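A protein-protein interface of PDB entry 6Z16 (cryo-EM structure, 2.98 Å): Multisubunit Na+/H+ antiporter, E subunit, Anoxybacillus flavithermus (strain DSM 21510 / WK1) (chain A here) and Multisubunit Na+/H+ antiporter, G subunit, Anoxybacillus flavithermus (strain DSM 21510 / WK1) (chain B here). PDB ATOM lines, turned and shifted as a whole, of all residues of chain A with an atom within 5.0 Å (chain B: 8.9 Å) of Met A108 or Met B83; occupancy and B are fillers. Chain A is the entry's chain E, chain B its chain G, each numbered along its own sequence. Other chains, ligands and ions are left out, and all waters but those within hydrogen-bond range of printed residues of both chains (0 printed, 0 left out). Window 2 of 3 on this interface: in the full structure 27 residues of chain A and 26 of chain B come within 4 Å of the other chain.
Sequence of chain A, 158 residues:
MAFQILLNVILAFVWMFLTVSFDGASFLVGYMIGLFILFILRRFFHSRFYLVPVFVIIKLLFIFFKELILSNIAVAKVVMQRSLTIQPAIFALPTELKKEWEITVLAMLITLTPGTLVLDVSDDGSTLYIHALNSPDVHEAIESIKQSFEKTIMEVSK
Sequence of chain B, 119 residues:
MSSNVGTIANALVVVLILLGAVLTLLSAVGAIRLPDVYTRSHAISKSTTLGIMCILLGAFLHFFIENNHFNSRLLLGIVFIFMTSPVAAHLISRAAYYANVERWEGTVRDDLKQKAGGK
CB of Phe A64 touches CZ of Phe B82, at 3.9 Å.
Thr A111 touches Lys B46 (O to CD, 3.9 Å).
Pro B86 touches Thr A111 (CB to CG2, 3.9 Å).
CE1 of Phe B82 touches CD1 of Leu A112, 3.6 Å away.
The backbone carbonyl oxygen (O) of Ala A107 lies within hydrogen-bond range of the side-chain hydroxyl (OG1) of Thr A111 (2.7 Å).
Of the 19 printed residues of chain B, 4 touch a printed residue of chain A.
Hydrophobic or aromatic side chains of chain B that line the printed part of chain A: Phe B82, Met B83 and Pro B86.
Among the printed residues, 5 pairs touch across the chains.
Among the printed residues, no Asp or Glu carboxylate lies within 4 Å of a Lys or Arg side-chain nitrogen of the other chain.
Met A108 touches one residue of chain B.
No residue of chain B comes within 4 Å of Ala A107.
Printed residues of chain A within 4 Å of Pro B86: Thr A111.
Of the printed residues of chain B, Thr A111 touches Lys B46 and Pro B86.
Printed residues of chain A within 4 Å of Lys B46: Thr A111.
Leu A106 touches none of the printed residues of chain B.
SD of Met B83 sits close to SD of Met A108 (3.6 Å).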
ATOM      1  N   PHE A  64       9.001  25.809  -6.383  1.00  0.00           N
ATOM      2  CA  PHE A  64       8.709  24.558  -5.674  1.00  0.00           C
ATOM      3  C   PHE A  64       9.350  24.529  -4.291  1.00  0.00           C
ATOM      4  O   PHE A  64       8.675  24.257  -3.288  1.00  0.00           O
ATOM      5  CB  PHE A  64       9.193  23.354  -6.484  1.00  0.00           C
ATOM      6  CG  PHE A  64       8.308  22.985  -7.636  1.00  0.00           C
ATOM      7  CD1 PHE A  64       7.018  23.470  -7.725  1.00  0.00           C
ATOM      8  CD2 PHE A  64       8.769  22.129  -8.624  1.00  0.00           C
ATOM      9  CE1 PHE A  64       6.203  23.124  -8.786  1.00  0.00           C
ATOM     10  CE2 PHE A  64       7.963  21.779  -9.688  1.00  0.00           C
ATOM     11  CZ  PHE A  64       6.672  22.278  -9.767  1.00  0.00           C
ATOM     12  N   THR A 104      -0.843  18.912 -14.695  1.00  0.00           N
ATOM     13  CA  THR A 104      -0.313  18.220 -13.529  1.00  0.00           C
ATOM     14  C   THR A 104       0.815  18.984 -12.848  1.00  0.00           C
ATOM     15  O   THR A 104       0.988  18.824 -11.637  1.00  0.00           O
ATOM     16  CB  THR A 104       0.141  16.794 -13.870  1.00  0.00           C
ATOM     17  OG1 THR A 104       0.428  16.090 -12.658  1.00  0.00           O
ATOM     18  CG2 THR A 104       1.379  16.792 -14.698  1.00  0.00           C
ATOM     19  N   VAL A 105       1.543  19.860 -13.552  1.00  0.00           N
ATOM     20  CA  VAL A 105       2.534  20.637 -12.812  1.00  0.00           C
ATOM     21  C   VAL A 105       1.846  21.778 -12.066  1.00  0.00           C
ATOM     22  O   VAL A 105       2.292  22.161 -10.977  1.00  0.00           O
ATOM     23  CB  VAL A 105       3.686  21.125 -13.717  1.00  0.00           C
ATOM     24  CG1 VAL A 105       3.270  22.259 -14.641  1.00  0.00           C
ATOM     25  CG2 VAL A 105       4.898  21.516 -12.883  1.00  0.00           C
ATOM     26  N   LEU A 106       0.705  22.265 -12.575  1.00  0.00           N
ATOM     27  CA  LEU A 106      -0.100  23.211 -11.814  1.00  0.00           C
ATOM     28  C   LEU A 106      -0.683  22.556 -10.576  1.00  0.00           C
ATOM     29  O   LEU A 106      -0.665  23.150  -9.496  1.00  0.00           O
ATOM     30  CB  LEU A 106      -1.215  23.786 -12.685  1.00  0.00           C
ATOM     31  CG  LEU A 106      -2.124  24.797 -11.982  1.00  0.00           C
ATOM     32  CD1 LEU A 106      -1.332  26.017 -11.562  1.00  0.00           C
ATOM     33  CD2 LEU A 106      -3.310  25.192 -12.845  1.00  0.00           C
ATOM     34  N   ALA A 107      -1.154  21.313 -10.706  1.00  0.00           N
ATOM     35  CA  ALA A 107      -1.721  20.605  -9.564  1.00  0.00           C
ATOM     36  C   ALA A 107      -0.656  20.259  -8.531  1.00  0.00           C
ATOM     37  O   ALA A 107      -0.903  20.357  -7.324  1.00  0.00           O
ATOM     38  CB  ALA A 107      -2.438  19.345 -10.039  1.00  0.00           C
ATOM     39  N   MET A 108       0.540  19.879  -8.982  1.00  0.00           N
ATOM     40  CA  MET A 108       1.602  19.528  -8.049  1.00  0.00           C
ATOM     41  C   MET A 108       2.192  20.766  -7.386  1.00  0.00           C
ATOM     42  O   MET A 108       2.690  20.688  -6.257  1.00  0.00           O
ATOM     43  CB  MET A 108       2.678  18.724  -8.778  1.00  0.00           C
ATOM     44  CG  MET A 108       3.698  18.050  -7.882  1.00  0.00           C
ATOM     45  SD  MET A 108       4.858  17.079  -8.852  1.00  0.00           S
ATOM     46  CE  MET A 108       3.772  15.776  -9.435  1.00  0.00           C
ATOM     47  N   LEU A 109       2.129  21.919  -8.055  1.00  0.00           N
ATOM     48  CA  LEU A 109       2.531  23.160  -7.408  1.00  0.00           C
ATOM     49  C   LEU A 109       1.481  23.645  -6.419  1.00  0.00           C
ATOM     50  O   LEU A 109       1.825  24.129  -5.337  1.00  0.00           O
ATOM     51  CB  LEU A 109       2.814  24.224  -8.469  1.00  0.00           C
ATOM     52  CG  LEU A 109       3.165  25.643  -8.029  1.00  0.00           C
ATOM     53  CD1 LEU A 109       4.293  25.652  -7.026  1.00  0.00           C
ATOM     54  CD2 LEU A 109       3.563  26.446  -9.251  1.00  0.00           C
ATOM     55  N   ILE A 110       0.201  23.513  -6.759  1.00  0.00           N
ATOM     56  CA  ILE A 110      -0.840  24.091  -5.924  1.00  0.00           C
ATOM     57  C   ILE A 110      -1.224  23.161  -4.777  1.00  0.00           C
ATOM     58  O   ILE A 110      -1.853  23.607  -3.811  1.00  0.00           O
ATOM     59  CB  ILE A 110      -2.026  24.461  -6.828  1.00  0.00           C
ATOM     60  CG1 ILE A 110      -2.935  25.496  -6.193  1.00  0.00           C
ATOM     61  CG2 ILE A 110      -2.861  23.280  -7.128  1.00  0.00           C
ATOM     62  CD1 ILE A 110      -3.959  25.988  -7.166  1.00  0.00           C
ATOM     63  N   THR A 111      -0.845  21.880  -4.845  1.00  0.00           N
ATOM     64  CA  THR A 111      -0.952  21.005  -3.680  1.00  0.00           C
ATOM     65  C   THR A 111       0.017  21.441  -2.593  1.00  0.00           C
ATOM     66  O   THR A 111      -0.357  21.586  -1.423  1.00  0.00           O
ATOM     67  CB  THR A 111      -0.663  19.557  -4.083  1.00  0.00           C
ATOM     68  OG1 THR A 111      -1.633  19.110  -5.033  1.00  0.00           O
ATOM     69  CG2 THR A 111      -0.677  18.637  -2.872  1.00  0.00           C
ATOM     70  N   LEU A 112       1.259  21.689  -2.979  1.00  0.00           N
ATOM     71  CA  LEU A 112       2.379  21.993  -2.106  1.00  0.00           C
ATOM     72  C   LEU A 112       2.402  23.458  -1.659  1.00  0.00           C
ATOM     73  O   LEU A 112       3.327  23.876  -0.961  1.00  0.00           O
ATOM     74  CB  LEU A 112       3.652  21.575  -2.846  1.00  0.00           C
ATOM     75  CG  LEU A 112       5.091  21.554  -2.359  1.00  0.00           C
ATOM     76  CD1 LEU A 112       5.748  20.317  -2.905  1.00  0.00           C
ATOM     77  CD2 LEU A 112       5.757  22.769  -2.939  1.00  0.00           C
ATOM     78  N   SER B  45       1.000  14.958   4.409  1.00  0.00           N
ATOM     79  CA  SER B  45       1.626  15.181   3.109  1.00  0.00           C
ATOM     80  C   SER B  45       2.786  16.162   3.155  1.00  0.00           C
ATOM     81  O   SER B  45       3.953  15.747   3.031  1.00  0.00           O
ATOM     82  CB  SER B  45       0.569  15.700   2.134  1.00  0.00           C
ATOM     83  OG  SER B  45       1.139  16.071   0.895  1.00  0.00           O
ATOM     84  N   LYS B  46       2.486  17.423   3.486  1.00  0.00           N
ATOM     85  CA  LYS B  46       3.514  18.448   3.373  1.00  0.00           C
ATOM     86  C   LYS B  46       4.582  18.297   4.451  1.00  0.00           C
ATOM     87  O   LYS B  46       5.789  18.352   4.147  1.00  0.00           O
ATOM     88  CB  LYS B  46       2.867  19.830   3.400  1.00  0.00           C
ATOM     89  CG  LYS B  46       1.954  20.037   2.201  1.00  0.00           C
ATOM     90  CD  LYS B  46       1.461  21.458   2.070  1.00  0.00           C
ATOM     91  CE  LYS B  46       0.348  21.806   3.026  1.00  0.00           C
ATOM     92  NZ  LYS B  46      -0.920  21.159   2.618  1.00  0.00           N
ATOM     93  N   THR B  49       6.753  15.032   4.126  1.00  0.00           N
ATOM     94  CA  THR B  49       7.564  15.133   2.916  1.00  0.00           C
ATOM     95  C   THR B  49       8.807  15.989   3.151  1.00  0.00           C
ATOM     96  O   THR B  49       9.939  15.557   2.871  1.00  0.00           O
ATOM     97  CB  THR B  49       6.712  15.700   1.781  1.00  0.00           C
ATOM     98  OG1 THR B  49       5.595  14.834   1.543  1.00  0.00           O
ATOM     99  CG2 THR B  49       7.512  15.815   0.515  1.00  0.00           C
ATOM    100  N   MET B  53      12.834  14.684   3.523  1.00  0.00           N
ATOM    101  CA  MET B  53      13.880  15.217   2.657  1.00  0.00           C
ATOM    102  C   MET B  53      14.981  15.907   3.449  1.00  0.00           C
ATOM    103  O   MET B  53      16.150  15.817   3.066  1.00  0.00           O
ATOM    104  CB  MET B  53      13.298  16.157   1.615  1.00  0.00           C
ATOM    105  CG  MET B  53      12.529  15.426   0.553  1.00  0.00           C
ATOM    106  SD  MET B  53      12.065  16.526  -0.781  1.00  0.00           S
ATOM    107  CE  MET B  53      10.790  17.443   0.040  1.00  0.00           C
ATOM    108  N   LEU B  76      18.511  10.624  -5.531  1.00  0.00           N
ATOM    109  CA  LEU B  76      17.381  10.118  -6.299  1.00  0.00           C
ATOM    110  C   LEU B  76      16.214   9.756  -5.394  1.00  0.00           C
ATOM    111  O   LEU B  76      15.053   9.894  -5.802  1.00  0.00           O
ATOM    112  CB  LEU B  76      17.796   8.928  -7.163  1.00  0.00           C
ATOM    113  CG  LEU B  76      18.311   9.313  -8.558  1.00  0.00           C
ATOM    114  CD1 LEU B  76      17.291  10.203  -9.257  1.00  0.00           C
ATOM    115  CD2 LEU B  76      19.695   9.960  -8.584  1.00  0.00           C
ATOM    116  N   GLY B  77      16.497   9.365  -4.149  1.00  0.00           N
ATOM    117  CA  GLY B  77      15.430   9.166  -3.183  1.00  0.00           C
ATOM    118  C   GLY B  77      14.716  10.452  -2.817  1.00  0.00           C
ATOM    119  O   GLY B  77      13.490  10.472  -2.694  1.00  0.00           O
ATOM    120  N   ILE B  78      15.474  11.539  -2.642  1.00  0.00           N
ATOM    121  CA  ILE B  78      14.886  12.845  -2.335  1.00  0.00           C
ATOM    122  C   ILE B  78      13.989  13.314  -3.475  1.00  0.00           C
ATOM    123  O   ILE B  78      12.851  13.753  -3.251  1.00  0.00           O
ATOM    124  CB  ILE B  78      15.996  13.867  -2.033  1.00  0.00           C
ATOM    125  CG1 ILE B  78      16.691  13.515  -0.727  1.00  0.00           C
ATOM    126  CG2 ILE B  78      15.441  15.264  -1.937  1.00  0.00           C
ATOM    127  CD1 ILE B  78      17.964  14.263  -0.504  1.00  0.00           C
ATOM    128  N   VAL B  79      14.474  13.185  -4.716  1.00  0.00           N
ATOM    129  CA  VAL B  79      13.680  13.589  -5.878  1.00  0.00           C
ATOM    130  C   VAL B  79      12.437  12.711  -6.020  1.00  0.00           C
ATOM    131  O   VAL B  79      11.340  13.207  -6.320  1.00  0.00           O
ATOM    132  CB  VAL B  79      14.555  13.568  -7.146  1.00  0.00           C
ATOM    133  CG1 VAL B  79      13.734  13.853  -8.397  1.00  0.00           C
ATOM    134  CG2 VAL B  79      15.676  14.582  -7.024  1.00  0.00           C
ATOM    135  N   PHE B  80      12.565  11.414  -5.714  1.00  0.00           N
ATOM    136  CA  PHE B  80      11.426  10.511  -5.824  1.00  0.00           C
ATOM    137  C   PHE B  80      10.355  10.812  -4.780  1.00  0.00           C
ATOM    138  O   PHE B  80       9.161  10.815  -5.101  1.00  0.00           O
ATOM    139  CB  PHE B  80      11.882   9.057  -5.698  1.00  0.00           C
ATOM    140  CG  PHE B  80      10.772   8.080  -5.899  1.00  0.00           C
ATOM    141  CD1 PHE B  80      10.338   7.777  -7.172  1.00  0.00           C
ATOM    142  CD2 PHE B  80      10.119   7.506  -4.819  1.00  0.00           C
ATOM    143  CE1 PHE B  80       9.304   6.904  -7.367  1.00  0.00           C
ATOM    144  CE2 PHE B  80       9.069   6.648  -5.013  1.00  0.00           C
ATOM    145  CZ  PHE B  80       8.665   6.339  -6.293  1.00  0.00           C
ATOM    146  N   ILE B  81      10.759  11.030  -3.524  1.00  0.00           N
ATOM    147  CA  ILE B  81       9.789  11.289  -2.463  1.00  0.00           C
ATOM    148  C   ILE B  81       9.085  12.618  -2.696  1.00  0.00           C
ATOM    149  O   ILE B  81       7.858  12.720  -2.534  1.00  0.00           O
ATOM    150  CB  ILE B  81      10.470  11.237  -1.081  1.00  0.00           C
ATOM    151  CG1 ILE B  81      10.996   9.835  -0.782  1.00  0.00           C
ATOM    152  CG2 ILE B  81       9.505  11.627  -0.001  1.00  0.00           C
ATOM    153  CD1 ILE B  81       9.933   8.771  -0.755  1.00  0.00           C
ATOM    154  N   PHE B  82       9.846  13.636  -3.135  1.00  0.00           N
ATOM    155  CA  PHE B  82       9.267  14.920  -3.521  1.00  0.00           C
ATOM    156  C   PHE B  82       8.260  14.768  -4.652  1.00  0.00           C
ATOM    157  O   PHE B  82       7.226  15.444  -4.666  1.00  0.00           O
ATOM    158  CB  PHE B  82      10.383  15.873  -3.940  1.00  0.00           C
ATOM    159  CG  PHE B  82       9.910  17.252  -4.298  1.00  0.00           C
ATOM    160  CD1 PHE B  82       9.597  18.168  -3.311  1.00  0.00           C
ATOM    161  CD2 PHE B  82       9.791  17.636  -5.626  1.00  0.00           C
ATOM    162  CE1 PHE B  82       9.174  19.440  -3.637  1.00  0.00           C
ATOM    163  CE2 PHE B  82       9.363  18.904  -5.958  1.00  0.00           C
ATOM    164  CZ  PHE B  82       9.055  19.807  -4.960  1.00  0.00           C
ATOM    165  N   MET B  83       8.534  13.875  -5.601  1.00  0.00           N
ATOM    166  CA  MET B  83       7.604  13.683  -6.706  1.00  0.00           C
ATOM    167  C   MET B  83       6.363  12.901  -6.284  1.00  0.00           C
ATOM    168  O   MET B  83       5.275  13.141  -6.818  1.00  0.00           O
ATOM    169  CB  MET B  83       8.323  12.971  -7.853  1.00  0.00           C
ATOM    170  CG  MET B  83       7.550  12.891  -9.156  1.00  0.00           C
ATOM    171  SD  MET B  83       7.237  14.521  -9.850  1.00  0.00           S
ATOM    172  CE  MET B  83       8.884  15.001 -10.356  1.00  0.00           C
ATOM    173  N   THR B  84       6.491  11.983  -5.323  1.00  0.00           N
ATOM    174  CA  THR B  84       5.466  10.963  -5.142  1.00  0.00           C
ATOM    175  C   THR B  84       4.601  11.079  -3.893  1.00  0.00           C
ATOM    176  O   THR B  84       3.500  10.522  -3.892  1.00  0.00           O
ATOM    177  CB  THR B  84       6.107   9.571  -5.157  1.00  0.00           C
ATOM    178  OG1 THR B  84       7.168   9.520  -4.197  1.00  0.00           O
ATOM    179  CG2 THR B  84       6.634   9.262  -6.535  1.00  0.00           C
ATOM    180  N   SER B  85       5.045  11.745  -2.830  1.00  0.00           N
ATOM    181  CA  SER B  85       4.133  11.770  -1.681  1.00  0.00           C
ATOM    182  C   SER B  85       2.922  12.722  -1.787  1.00  0.00           C
ATOM    183  O   SER B  85       1.837  12.338  -1.312  1.00  0.00           O
ATOM    184  CB  SER B  85       4.921  12.013  -0.385  1.00  0.00           C
ATOM    185  OG  SER B  85       5.605  13.242  -0.351  1.00  0.00           O
ATOM    186  N   PRO B  86       3.001  13.929  -2.385  1.00  0.00           N
ATOM    187  CA  PRO B  86       1.760  14.707  -2.529  1.00  0.00           C
ATOM    188  C   PRO B  86       0.778  14.135  -3.534  1.00  0.00           C
ATOM    189  O   PRO B  86      -0.430  14.332  -3.361  1.00  0.00           O
ATOM    190  CB  PRO B  86       2.255  16.091  -2.964  1.00  0.00           C
ATOM    191  CG  PRO B  86       3.619  16.157  -2.509  1.00  0.00           C
ATOM    192  CD  PRO B  86       4.151  14.797  -2.708  1.00  0.00           C
ATOM    193  N   VAL B  87       1.235  13.424  -4.566  1.00  0.00           N
ATOM    194  CA  VAL B  87       0.271  12.792  -5.462  1.00  0.00           C
ATOM    195  C   VAL B  87      -0.370  11.588  -4.774  1.00  0.00           C
ATOM    196  O   VAL B  87      -1.534  11.254  -5.043  1.00  0.00           O
ATOM    197  CB  VAL B  87       0.933  12.440  -6.814  1.00  0.00           C
ATOM    198  CG1 VAL B  87       2.016  11.401  -6.664  1.00  0.00           C
ATOM    199  CG2 VAL B  87      -0.098  11.982  -7.830  1.00  0.00           C
ATOM    200  N   ALA B  88       0.337  10.975  -3.820  1.00  0.00           N
ATOM    201  CA  ALA B  88      -0.270   9.944  -2.987  1.00  0.00           C
ATOM    202  C   ALA B  88      -1.381  10.529  -2.125  1.00  0.00           C
ATOM    203  O   ALA B  88      -2.481   9.966  -2.049  1.00  0.00           O
ATOM    204  CB  ALA B  88       0.794   9.279  -2.117  1.00  0.00           C
ATOM    205  N   ALA B  89      -1.116  11.682  -1.498  1.00  0.00           N
ATOM    206  CA  ALA B  89      -2.143  12.352  -0.703  1.00  0.00           C
ATOM    207  C   ALA B  89      -3.323  12.797  -1.559  1.00  0.00           C
ATOM    208  O   ALA B  89      -4.476  12.712  -1.124  1.00  0.00           O
ATOM    209  CB  ALA B  89      -1.542  13.545   0.027  1.00  0.00           C
ATOM    210  N   HIS B  90      -3.047  13.251  -2.787  1.00  0.00           N
ATOM    211  CA  HIS B  90      -4.099  13.591  -3.742  1.00  0.00           C
ATOM    212  C   HIS B  90      -4.984  12.397  -4.067  1.00  0.00           C
ATOM    213  O   HIS B  90      -6.214  12.525  -4.122  1.00  0.00           O
ATOM    214  CB  HIS B  90      -3.479  14.137  -5.027  1.00  0.00           C
ATOM    215  CG  HIS B  90      -4.471  14.371  -6.123  1.00  0.00           C
ATOM    216  ND1 HIS B  90      -4.798  13.405  -7.049  1.00  0.00           N
ATOM    217  CD2 HIS B  90      -5.222  15.452  -6.431  1.00  0.00           C
ATOM    218  CE1 HIS B  90      -5.700  13.884  -7.885  1.00  0.00           C
ATOM    219  NE2 HIS B  90      -5.975  15.124  -7.530  1.00  0.00           N
